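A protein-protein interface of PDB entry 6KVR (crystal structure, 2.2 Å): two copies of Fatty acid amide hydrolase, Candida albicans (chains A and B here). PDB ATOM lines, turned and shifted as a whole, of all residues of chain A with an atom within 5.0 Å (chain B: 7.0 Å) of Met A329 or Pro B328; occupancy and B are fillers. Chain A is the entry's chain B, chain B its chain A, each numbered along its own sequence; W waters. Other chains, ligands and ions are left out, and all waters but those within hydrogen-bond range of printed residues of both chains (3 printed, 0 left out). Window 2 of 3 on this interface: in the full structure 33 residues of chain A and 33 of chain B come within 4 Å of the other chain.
NH1 of Arg A549 lies within hydrogen-bond range of O of Ser B324 (2.9 Å).
Pro B328 touches just these residues of chain A: Met A329, Arg A549 and Tyr A550. Of the printed residues of chain B, Arg A549 touches Ser B324 (2.9 Å) and Pro B328 (3.95 Å). Printed residues of chain A within 4 Å of Tyr B550: Leu A327 and Pro A328. Of the printed residues of chain A, Met B329 touches Met A329. Of the printed residues of chain B, Pro A328 touches Tyr B550. Thr B325 touches none of the printed residues of chain A. The nearest residue of chain B that does not touch Met A329 is Leu B327 (4.5 Å). The nearest printed residue of chain A that does not touch Tyr B550 is Met A329 (6.8 Å).
Water W3 bridges O of Thr B325 and NH1 of Arg A549. Water W2 lies within hydrogen-bond range of the backbone carbonyl oxygen of Pro B328 (2.8 Å) and the side-chain sulfur of Met A329 (3.8 Å). Water W1 bridges the backbone carbonyl oxygen of Pro A328 (3.0 Å) and the side-chain sulfur of Met B329 (3.8 Å).
The backbone NH of Leu B327 sits at hydrogen-bond distance from the backbone carbonyl oxygen of Lys B275 (2.8 Å). NH2 of Arg A276 sits at hydrogen-bond distance from O of Met A329 (3.5 Å).
Leu A327 touches its own counterpart, Leu B327. Leu A327 touches Tyr B550, and with the chains exchanged Tyr A550 touches Leu B327. Met A329 touches Pro B328, but with the chains exchanged Pro A328 does not touch Met B329 (4.01 Å). Met A329 touches its own counterpart, Met B329.
Of the 12 printed residues of chain B, 5 touch a printed residue of chain A. Hydrophobic or aromatic side chains of chain B that line the printed part of chain A: Leu B327, Pro B328, Met B329 and Tyr B550. Of the 11 printed residues of chain A, 5 touch a printed residue of chain B. Hydrophobic or aromatic side chains of chain A that line the printed part of chain B: Leu A327, Pro A328, Met A329 and Tyr A550. Among the printed residues, no Asp or Glu carboxylate lies within 4 Å of a Lys or Arg side-chain nitrogen of the other chain.
Leu A327 touches Leu B327. CD2 of Leu A327 touches CE2 of Tyr B550, at 3.4 Å. Pro A328 touches Tyr B550 (CG to CB, 3.5 Å). O of Pro B328 touches CE of Met A329 (3.3 Å). Met A329 touches Met B329. Pro B328 touches Arg A549 (CG to O, 3.95 Å). CD2 of Leu B327 touches CE2 of Tyr A550, at 3.4 Å. Tyr A550 touches Pro B328.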
ATOM      1  N   ARG A 276      -5.337  15.885  19.836  1.00  0.00           N
ATOM      2  CA  ARG A 276      -5.720  16.018  21.232  1.00  0.00           C
ATOM      3  C   ARG A 276      -6.542  17.287  21.451  1.00  0.00           C
ATOM      4  O   ARG A 276      -7.626  17.230  22.038  1.00  0.00           O
ATOM      5  CB  ARG A 276      -4.469  15.985  22.115  1.00  0.00           C
ATOM      6  CG  ARG A 276      -3.659  14.706  21.924  1.00  0.00           C
ATOM      7  CD  ARG A 276      -2.610  14.499  23.019  1.00  0.00           C
ATOM      8  NE  ARG A 276      -3.188  13.887  24.209  1.00  0.00           N
ATOM      9  CZ  ARG A 276      -2.478  13.403  25.223  1.00  0.00           C
ATOM     10  NH1 ARG A 276      -1.154  13.417  25.212  1.00  0.00           N
ATOM     11  NH2 ARG A 276      -3.113  12.879  26.267  1.00  0.00           N
ATOM     12  N   ILE A 314      -8.595  18.710  28.286  1.00  0.00           N
ATOM     13  CA  ILE A 314      -8.865  17.333  27.862  1.00  0.00           C
ATOM     14  C   ILE A 314      -9.813  16.631  28.832  1.00  0.00           C
ATOM     15  O   ILE A 314     -10.891  16.161  28.441  1.00  0.00           O
ATOM     16  CB  ILE A 314      -7.539  16.562  27.700  1.00  0.00           C
ATOM     17  CG1 ILE A 314      -6.699  17.213  26.597  1.00  0.00           C
ATOM     18  CG2 ILE A 314      -7.779  15.120  27.358  1.00  0.00           C
ATOM     19  CD1 ILE A 314      -5.313  16.636  26.450  1.00  0.00           C
ATOM     20  N   TRP A 320     -13.755  15.441  22.447  1.00  0.00           N
ATOM     21  CA  TRP A 320     -14.364  14.445  21.570  1.00  0.00           C
ATOM     22  C   TRP A 320     -15.886  14.469  21.596  1.00  0.00           C
ATOM     23  O   TRP A 320     -16.514  13.885  20.707  1.00  0.00           O
ATOM     24  CB  TRP A 320     -13.878  13.050  21.946  1.00  0.00           C
ATOM     25  CG  TRP A 320     -14.089  12.711  23.383  1.00  0.00           C
ATOM     26  CD1 TRP A 320     -15.139  12.017  23.918  1.00  0.00           C
ATOM     27  CD2 TRP A 320     -13.225  13.035  24.476  1.00  0.00           C
ATOM     28  NE1 TRP A 320     -14.981  11.891  25.276  1.00  0.00           N
ATOM     29  CE2 TRP A 320     -13.814  12.508  25.645  1.00  0.00           C
ATOM     30  CE3 TRP A 320     -12.001  13.712  24.582  1.00  0.00           C
ATOM     31  CZ2 TRP A 320     -13.223  12.638  26.905  1.00  0.00           C
ATOM     32  CZ3 TRP A 320     -11.414  13.837  25.840  1.00  0.00           C
ATOM     33  CH2 TRP A 320     -12.029  13.303  26.979  1.00  0.00           C
ATOM     34  N   LEU A 327      -9.252  12.978  19.989  1.00  0.00           N
ATOM     35  CA  LEU A 327      -9.163  11.661  20.584  1.00  0.00           C
ATOM     36  C   LEU A 327      -9.653  11.688  22.027  1.00  0.00           C
ATOM     37  O   LEU A 327      -9.269  12.573  22.783  1.00  0.00           O
ATOM     38  CB  LEU A 327      -7.728  11.169  20.565  1.00  0.00           C
ATOM     39  CG  LEU A 327      -7.075  10.921  19.219  1.00  0.00           C
ATOM     40  CD1 LEU A 327      -5.593  10.602  19.446  1.00  0.00           C
ATOM     41  CD2 LEU A 327      -7.794   9.777  18.492  1.00  0.00           C
ATOM     42  N   PRO A 328     -10.471  10.701  22.455  1.00  0.00           N
ATOM     43  CA  PRO A 328     -10.763  10.553  23.897  1.00  0.00           C
ATOM     44  C   PRO A 328      -9.589   9.906  24.620  1.00  0.00           C
ATOM     45  O   PRO A 328      -9.633   8.770  25.094  1.00  0.00           O
ATOM     46  CB  PRO A 328     -12.014   9.670  23.895  1.00  0.00           C
ATOM     47  CG  PRO A 328     -11.878   8.842  22.715  1.00  0.00           C
ATOM     48  CD  PRO A 328     -11.155   9.678  21.656  1.00  0.00           C
ATOM     49  N   MET A 329      -8.478  10.628  24.678  1.00  0.00           N
ATOM     50  CA  MET A 329      -7.283  10.078  25.306  1.00  0.00           C
ATOM     51  C   MET A 329      -6.910  10.876  26.553  1.00  0.00           C
ATOM     52  O   MET A 329      -6.485  12.037  26.451  1.00  0.00           O
ATOM     53  CB  MET A 329      -6.129  10.026  24.307  1.00  0.00           C
ATOM     54  CG  MET A 329      -4.814   9.636  24.935  1.00  0.00           C
ATOM     55  SD  MET A 329      -3.276   9.777  23.727  1.00  0.00           S
ATOM     56  CE  MET A 329      -3.356   7.983  23.016  1.00  0.00           C
ATOM     57  N   PRO A 330      -7.069  10.228  27.714  1.00  0.00           N
ATOM     58  CA  PRO A 330      -6.962  10.941  28.993  1.00  0.00           C
ATOM     59  C   PRO A 330      -5.630  11.656  29.117  1.00  0.00           C
ATOM     60  O   PRO A 330      -4.595  11.157  28.665  1.00  0.00           O
ATOM     61  CB  PRO A 330      -7.091   9.816  30.035  1.00  0.00           C
ATOM     62  CG  PRO A 330      -7.800   8.693  29.326  1.00  0.00           C
ATOM     63  CD  PRO A 330      -7.314   8.787  27.895  1.00  0.00           C
ATOM     64  N   TRP A 331      -5.664  12.852  29.703  1.00  0.00           N
ATOM     65  CA  TRP A 331      -4.428  13.540  30.055  1.00  0.00           C
ATOM     66  C   TRP A 331      -3.913  12.882  31.327  1.00  0.00           C
ATOM     67  O   TRP A 331      -4.566  12.944  32.372  1.00  0.00           O
ATOM     68  CB  TRP A 331      -4.652  15.038  30.247  1.00  0.00           C
ATOM     69  CG  TRP A 331      -3.393  15.756  30.645  1.00  0.00           C
ATOM     70  CD1 TRP A 331      -3.003  16.085  31.913  1.00  0.00           C
ATOM     71  CD2 TRP A 331      -2.336  16.201  29.774  1.00  0.00           C
ATOM     72  NE1 TRP A 331      -1.776  16.707  31.888  1.00  0.00           N
ATOM     73  CE2 TRP A 331      -1.346  16.796  30.589  1.00  0.00           C
ATOM     74  CE3 TRP A 331      -2.128  16.146  28.388  1.00  0.00           C
ATOM     75  CZ2 TRP A 331      -0.169  17.338  30.064  1.00  0.00           C
ATOM     76  CZ3 TRP A 331      -0.960  16.681  27.867  1.00  0.00           C
ATOM     77  CH2 TRP A 331       0.005  17.276  28.707  1.00  0.00           C
ATOM     78  N   ARG A 549       5.466  10.438  20.168  1.00  0.00           N
ATOM     79  CA  ARG A 549       4.076  10.785  19.876  1.00  0.00           C
ATOM     80  C   ARG A 549       3.146  10.346  21.010  1.00  0.00           C
ATOM     81  O   ARG A 549       3.244   9.221  21.515  1.00  0.00           O
ATOM     82  CB  ARG A 549       3.632  10.152  18.545  1.00  0.00           C
ATOM     83  CG  ARG A 549       4.480  10.539  17.337  1.00  0.00           C
ATOM     84  CD  ARG A 549       3.858  10.074  16.021  1.00  0.00           C
ATOM     85  NE  ARG A 549       2.709  10.892  15.647  1.00  0.00           N
ATOM     86  CZ  ARG A 549       1.537  10.403  15.281  1.00  0.00           C
ATOM     87  NH1 ARG A 549       1.324   9.093  15.219  1.00  0.00           N
ATOM     88  NH2 ARG A 549       0.555  11.241  14.971  1.00  0.00           N
ATOM     89  N   TYR A 550       2.256  11.261  21.411  1.00  0.00           N
ATOM     90  CA  TYR A 550       1.261  11.072  22.463  1.00  0.00           C
ATOM     91  C   TYR A 550       1.881  10.918  23.852  1.00  0.00           C
ATOM     92  O   TYR A 550       1.183  10.562  24.804  1.00  0.00           O
ATOM     93  CB  TYR A 550       0.316   9.912  22.115  1.00  0.00           C
ATOM     94  CG  TYR A 550      -0.443  10.278  20.857  1.00  0.00           C
ATOM     95  CD1 TYR A 550      -1.463  11.212  20.907  1.00  0.00           C
ATOM     96  CD2 TYR A 550      -0.078   9.763  19.613  1.00  0.00           C
ATOM     97  CE1 TYR A 550      -2.134  11.604  19.768  1.00  0.00           C
ATOM     98  CE2 TYR A 550      -0.748  10.151  18.451  1.00  0.00           C
ATOM     99  CZ  TYR A 550      -1.770  11.082  18.539  1.00  0.00           C
ATOM    100  OH  TYR A 550      -2.454  11.503  17.407  1.00  0.00           O
ATOM    101  N   PHE A 551       3.161  11.254  24.011  1.00  0.00           N
ATOM    102  CA  PHE A 551       3.763  11.411  25.337  1.00  0.00           C
ATOM    103  C   PHE A 551       3.893  12.884  25.735  1.00  0.00           C
ATOM    104  O   PHE A 551       4.879  13.290  26.366  1.00  0.00           O
ATOM    105  CB  PHE A 551       5.115  10.712  25.386  1.00  0.00           C
ATOM    106  CG  PHE A 551       5.010   9.213  25.434  1.00  0.00           C
ATOM    107  CD1 PHE A 551       5.270   8.521  26.615  1.00  0.00           C
ATOM    108  CD2 PHE A 551       4.658   8.493  24.302  1.00  0.00           C
ATOM    109  CE1 PHE A 551       5.173   7.135  26.668  1.00  0.00           C
ATOM    110  CE2 PHE A 551       4.556   7.108  24.339  1.00  0.00           C
ATOM    111  CZ  PHE A 551       4.817   6.426  25.523  1.00  0.00           C
ATOM    112  N   LYS B 275      -6.232   3.143  13.882  1.00  0.00           N
ATOM    113  CA  LYS B 275      -4.978   3.488  14.545  1.00  0.00           C
ATOM    114  C   LYS B 275      -4.830   2.871  15.927  1.00  0.00           C
ATOM    115  O   LYS B 275      -4.013   3.321  16.714  1.00  0.00           O
ATOM    116  CB  LYS B 275      -4.779   5.006  14.608  1.00  0.00           C
ATOM    117  CG  LYS B 275      -4.902   5.675  13.229  1.00  0.00           C
ATOM    118  CD  LYS B 275      -5.722   6.961  13.297  1.00  0.00           C
ATOM    119  CE  LYS B 275      -4.826   8.227  13.298  1.00  0.00           C
ATOM    120  NZ  LYS B 275      -5.487   9.478  13.839  1.00  0.00           N
ATOM    121  N   ILE B 314      -2.811  -4.737  22.415  1.00  0.00           N
ATOM    122  CA  ILE B 314      -2.531  -3.343  22.720  1.00  0.00           C
ATOM    123  C   ILE B 314      -1.708  -3.215  23.999  1.00  0.00           C
ATOM    124  O   ILE B 314      -0.637  -2.594  24.000  1.00  0.00           O
ATOM    125  CB  ILE B 314      -3.850  -2.557  22.812  1.00  0.00           C
ATOM    126  CG1 ILE B 314      -4.494  -2.434  21.428  1.00  0.00           C
ATOM    127  CG2 ILE B 314      -3.634  -1.194  23.499  1.00  0.00           C
ATOM    128  CD1 ILE B 314      -5.968  -2.051  21.467  1.00  0.00           C
ATOM    129  N   PRO B 319       1.924  -1.730  20.136  1.00  0.00           N
ATOM    130  CA  PRO B 319       2.285  -1.531  18.722  1.00  0.00           C
ATOM    131  C   PRO B 319       2.933  -0.179  18.429  1.00  0.00           C
ATOM    132  O   PRO B 319       3.729  -0.081  17.480  1.00  0.00           O
ATOM    133  CB  PRO B 319       0.939  -1.661  18.000  1.00  0.00           C
ATOM    134  CG  PRO B 319      -0.064  -1.307  19.024  1.00  0.00           C
ATOM    135  CD  PRO B 319       0.466  -1.811  20.320  1.00  0.00           C
ATOM    136  N   TRP B 320       2.605   0.869  19.199  1.00  0.00           N
ATOM    137  CA  TRP B 320       3.241   2.166  18.991  1.00  0.00           C
ATOM    138  C   TRP B 320       4.756   2.082  19.119  1.00  0.00           C
ATOM    139  O   TRP B 320       5.456   2.940  18.574  1.00  0.00           O
ATOM    140  CB  TRP B 320       2.690   3.218  19.973  1.00  0.00           C
ATOM    141  CG  TRP B 320       2.831   2.810  21.393  1.00  0.00           C
ATOM    142  CD1 TRP B 320       3.873   3.094  22.229  1.00  0.00           C
ATOM    143  CD2 TRP B 320       1.912   2.008  22.151  1.00  0.00           C
ATOM    144  NE1 TRP B 320       3.659   2.524  23.463  1.00  0.00           N
ATOM    145  CE2 TRP B 320       2.462   1.855  23.444  1.00  0.00           C
ATOM    146  CE3 TRP B 320       0.677   1.412  21.866  1.00  0.00           C
ATOM    147  CZ2 TRP B 320       1.815   1.134  24.453  1.00  0.00           C
ATOM    148  CZ3 TRP B 320       0.029   0.692  22.876  1.00  0.00           C
ATOM    149  CH2 TRP B 320       0.603   0.557  24.149  1.00  0.00           C
ATOM    150  N   SER B 324       4.698   3.858  14.317  1.00  0.00           N
ATOM    151  CA  SER B 324       4.479   5.204  14.827  1.00  0.00           C
ATOM    152  C   SER B 324       3.031   5.655  14.653  1.00  0.00           C
ATOM    153  O   SER B 324       2.557   6.503  15.418  1.00  0.00           O
ATOM    154  CB  SER B 324       5.427   6.169  14.117  1.00  0.00           C
ATOM    155  OG  SER B 324       5.318   7.451  14.699  1.00  0.00           O
ATOM    156  N   THR B 325       2.318   5.110  13.656  1.00  0.00           N
ATOM    157  CA  THR B 325       0.907   5.433  13.444  1.00  0.00           C
ATOM    158  C   THR B 325       0.020   4.904  14.570  1.00  0.00           C
ATOM    159  O   THR B 325      -1.057   5.462  14.828  1.00  0.00           O
ATOM    160  CB  THR B 325       0.442   4.840  12.109  1.00  0.00           C
ATOM    161  OG1 THR B 325       1.267   5.337  11.051  1.00  0.00           O
ATOM    162  CG2 THR B 325      -1.016   5.192  11.821  1.00  0.00           C
ATOM    163  N   SER B 326       0.436   3.833  15.241  1.00  0.00           N
ATOM    164  CA  SER B 326      -0.426   3.221  16.243  1.00  0.00           C
ATOM    165  C   SER B 326      -0.481   4.072  17.508  1.00  0.00           C
ATOM    166  O   SER B 326       0.549   4.529  18.009  1.00  0.00           O
ATOM    167  CB  SER B 326       0.065   1.814  16.564  1.00  0.00           C
ATOM    168  OG  SER B 326      -0.229   0.941  15.485  1.00  0.00           O
ATOM    169  N   LEU B 327      -1.688   4.268  18.032  1.00  0.00           N
ATOM    170  CA  LEU B 327      -1.913   5.137  19.173  1.00  0.00           C
ATOM    171  C   LEU B 327      -1.589   4.413  20.479  1.00  0.00           C
ATOM    172  O   LEU B 327      -1.962   3.251  20.659  1.00  0.00           O
ATOM    173  CB  LEU B 327      -3.365   5.614  19.212  1.00  0.00           C
ATOM    174  CG  LEU B 327      -3.917   6.478  18.073  1.00  0.00           C
ATOM    175  CD1 LEU B 327      -5.382   6.834  18.348  1.00  0.00           C
ATOM    176  CD2 LEU B 327      -3.079   7.735  17.880  1.00  0.00           C
ATOM    177  N   PRO B 328      -0.900   5.078  21.415  1.00  0.00           N
ATOM    178  CA  PRO B 328      -0.730   4.505  22.760  1.00  0.00           C
ATOM    179  C   PRO B 328      -1.917   4.844  23.658  1.00  0.00           C
ATOM    180  O   PRO B 328      -1.801   5.577  24.638  1.00  0.00           O
ATOM    181  CB  PRO B 328       0.577   5.148  23.233  1.00  0.00           C
ATOM    182  CG  PRO B 328       0.618   6.446  22.537  1.00  0.00           C
ATOM    183  CD  PRO B 328      -0.055   6.264  21.206  1.00  0.00           C
ATOM    184  N   MET B 329      -3.085   4.334  23.292  1.00  0.00           N
ATOM    185  CA  MET B 329      -4.250   4.513  24.129  1.00  0.00           C
ATOM    186  C   MET B 329      -4.634   3.147  24.687  1.00  0.00           C
ATOM    187  O   MET B 329      -4.953   2.211  23.943  1.00  0.00           O
ATOM    188  CB  MET B 329      -5.356   5.224  23.351  1.00  0.00           C
ATOM    189  CG  MET B 329      -6.300   4.442  22.473  1.00  0.00           C
ATOM    190  SD  MET B 329      -8.045   5.347  22.567  1.00  0.00           S
ATOM    191  CE  MET B 329      -7.497   7.187  22.088  1.00  0.00           C
ATOM    192  N   PRO B 330      -4.509   3.027  26.005  1.00  0.00           N
ATOM    193  CA  PRO B 330      -4.669   1.723  26.660  1.00  0.00           C
ATOM    194  C   PRO B 330      -6.029   1.114  26.373  1.00  0.00           C
ATOM    195  O   PRO B 330      -7.029   1.819  26.229  1.00  0.00           O
ATOM    196  CB  PRO B 330      -4.526   2.055  28.151  1.00  0.00           C
ATOM    197  CG  PRO B 330      -3.745   3.367  28.175  1.00  0.00           C
ATOM    198  CD  PRO B 330      -4.162   4.108  26.944  1.00  0.00           C
ATOM    199  N   TYR B 550     -13.414   5.266  19.278  1.00  0.00           N
ATOM    200  CA  TYR B 550     -12.459   4.889  20.324  1.00  0.00           C
ATOM    201  C   TYR B 550     -13.128   4.341  21.575  1.00  0.00           C
ATOM    202  O   TYR B 550     -12.477   4.196  22.611  1.00  0.00           O
ATOM    203  CB  TYR B 550     -11.509   6.045  20.667  1.00  0.00           C
ATOM    204  CG  TYR B 550     -10.647   6.329  19.472  1.00  0.00           C
ATOM    205  CD1 TYR B 550      -9.604   5.472  19.133  1.00  0.00           C
ATOM    206  CD2 TYR B 550     -10.929   7.397  18.627  1.00  0.00           C
ATOM    207  CE1 TYR B 550      -8.834   5.696  18.014  1.00  0.00           C
ATOM    208  CE2 TYR B 550     -10.167   7.630  17.497  1.00  0.00           C
ATOM    209  CZ  TYR B 550      -9.125   6.777  17.194  1.00  0.00           C
ATOM    210  OH  TYR B 550      -8.375   7.009  16.064  1.00  0.00           O
HETATM  211  O   HOH W   1      -9.520   5.929  25.988  1.00  0.00           O
HETATM  212  O   HOH W   2      -2.062   7.626  26.571  1.00  0.00           O
HETATM  213  O   HOH W   3      -1.207   8.099  14.145  1.00  0.00           O
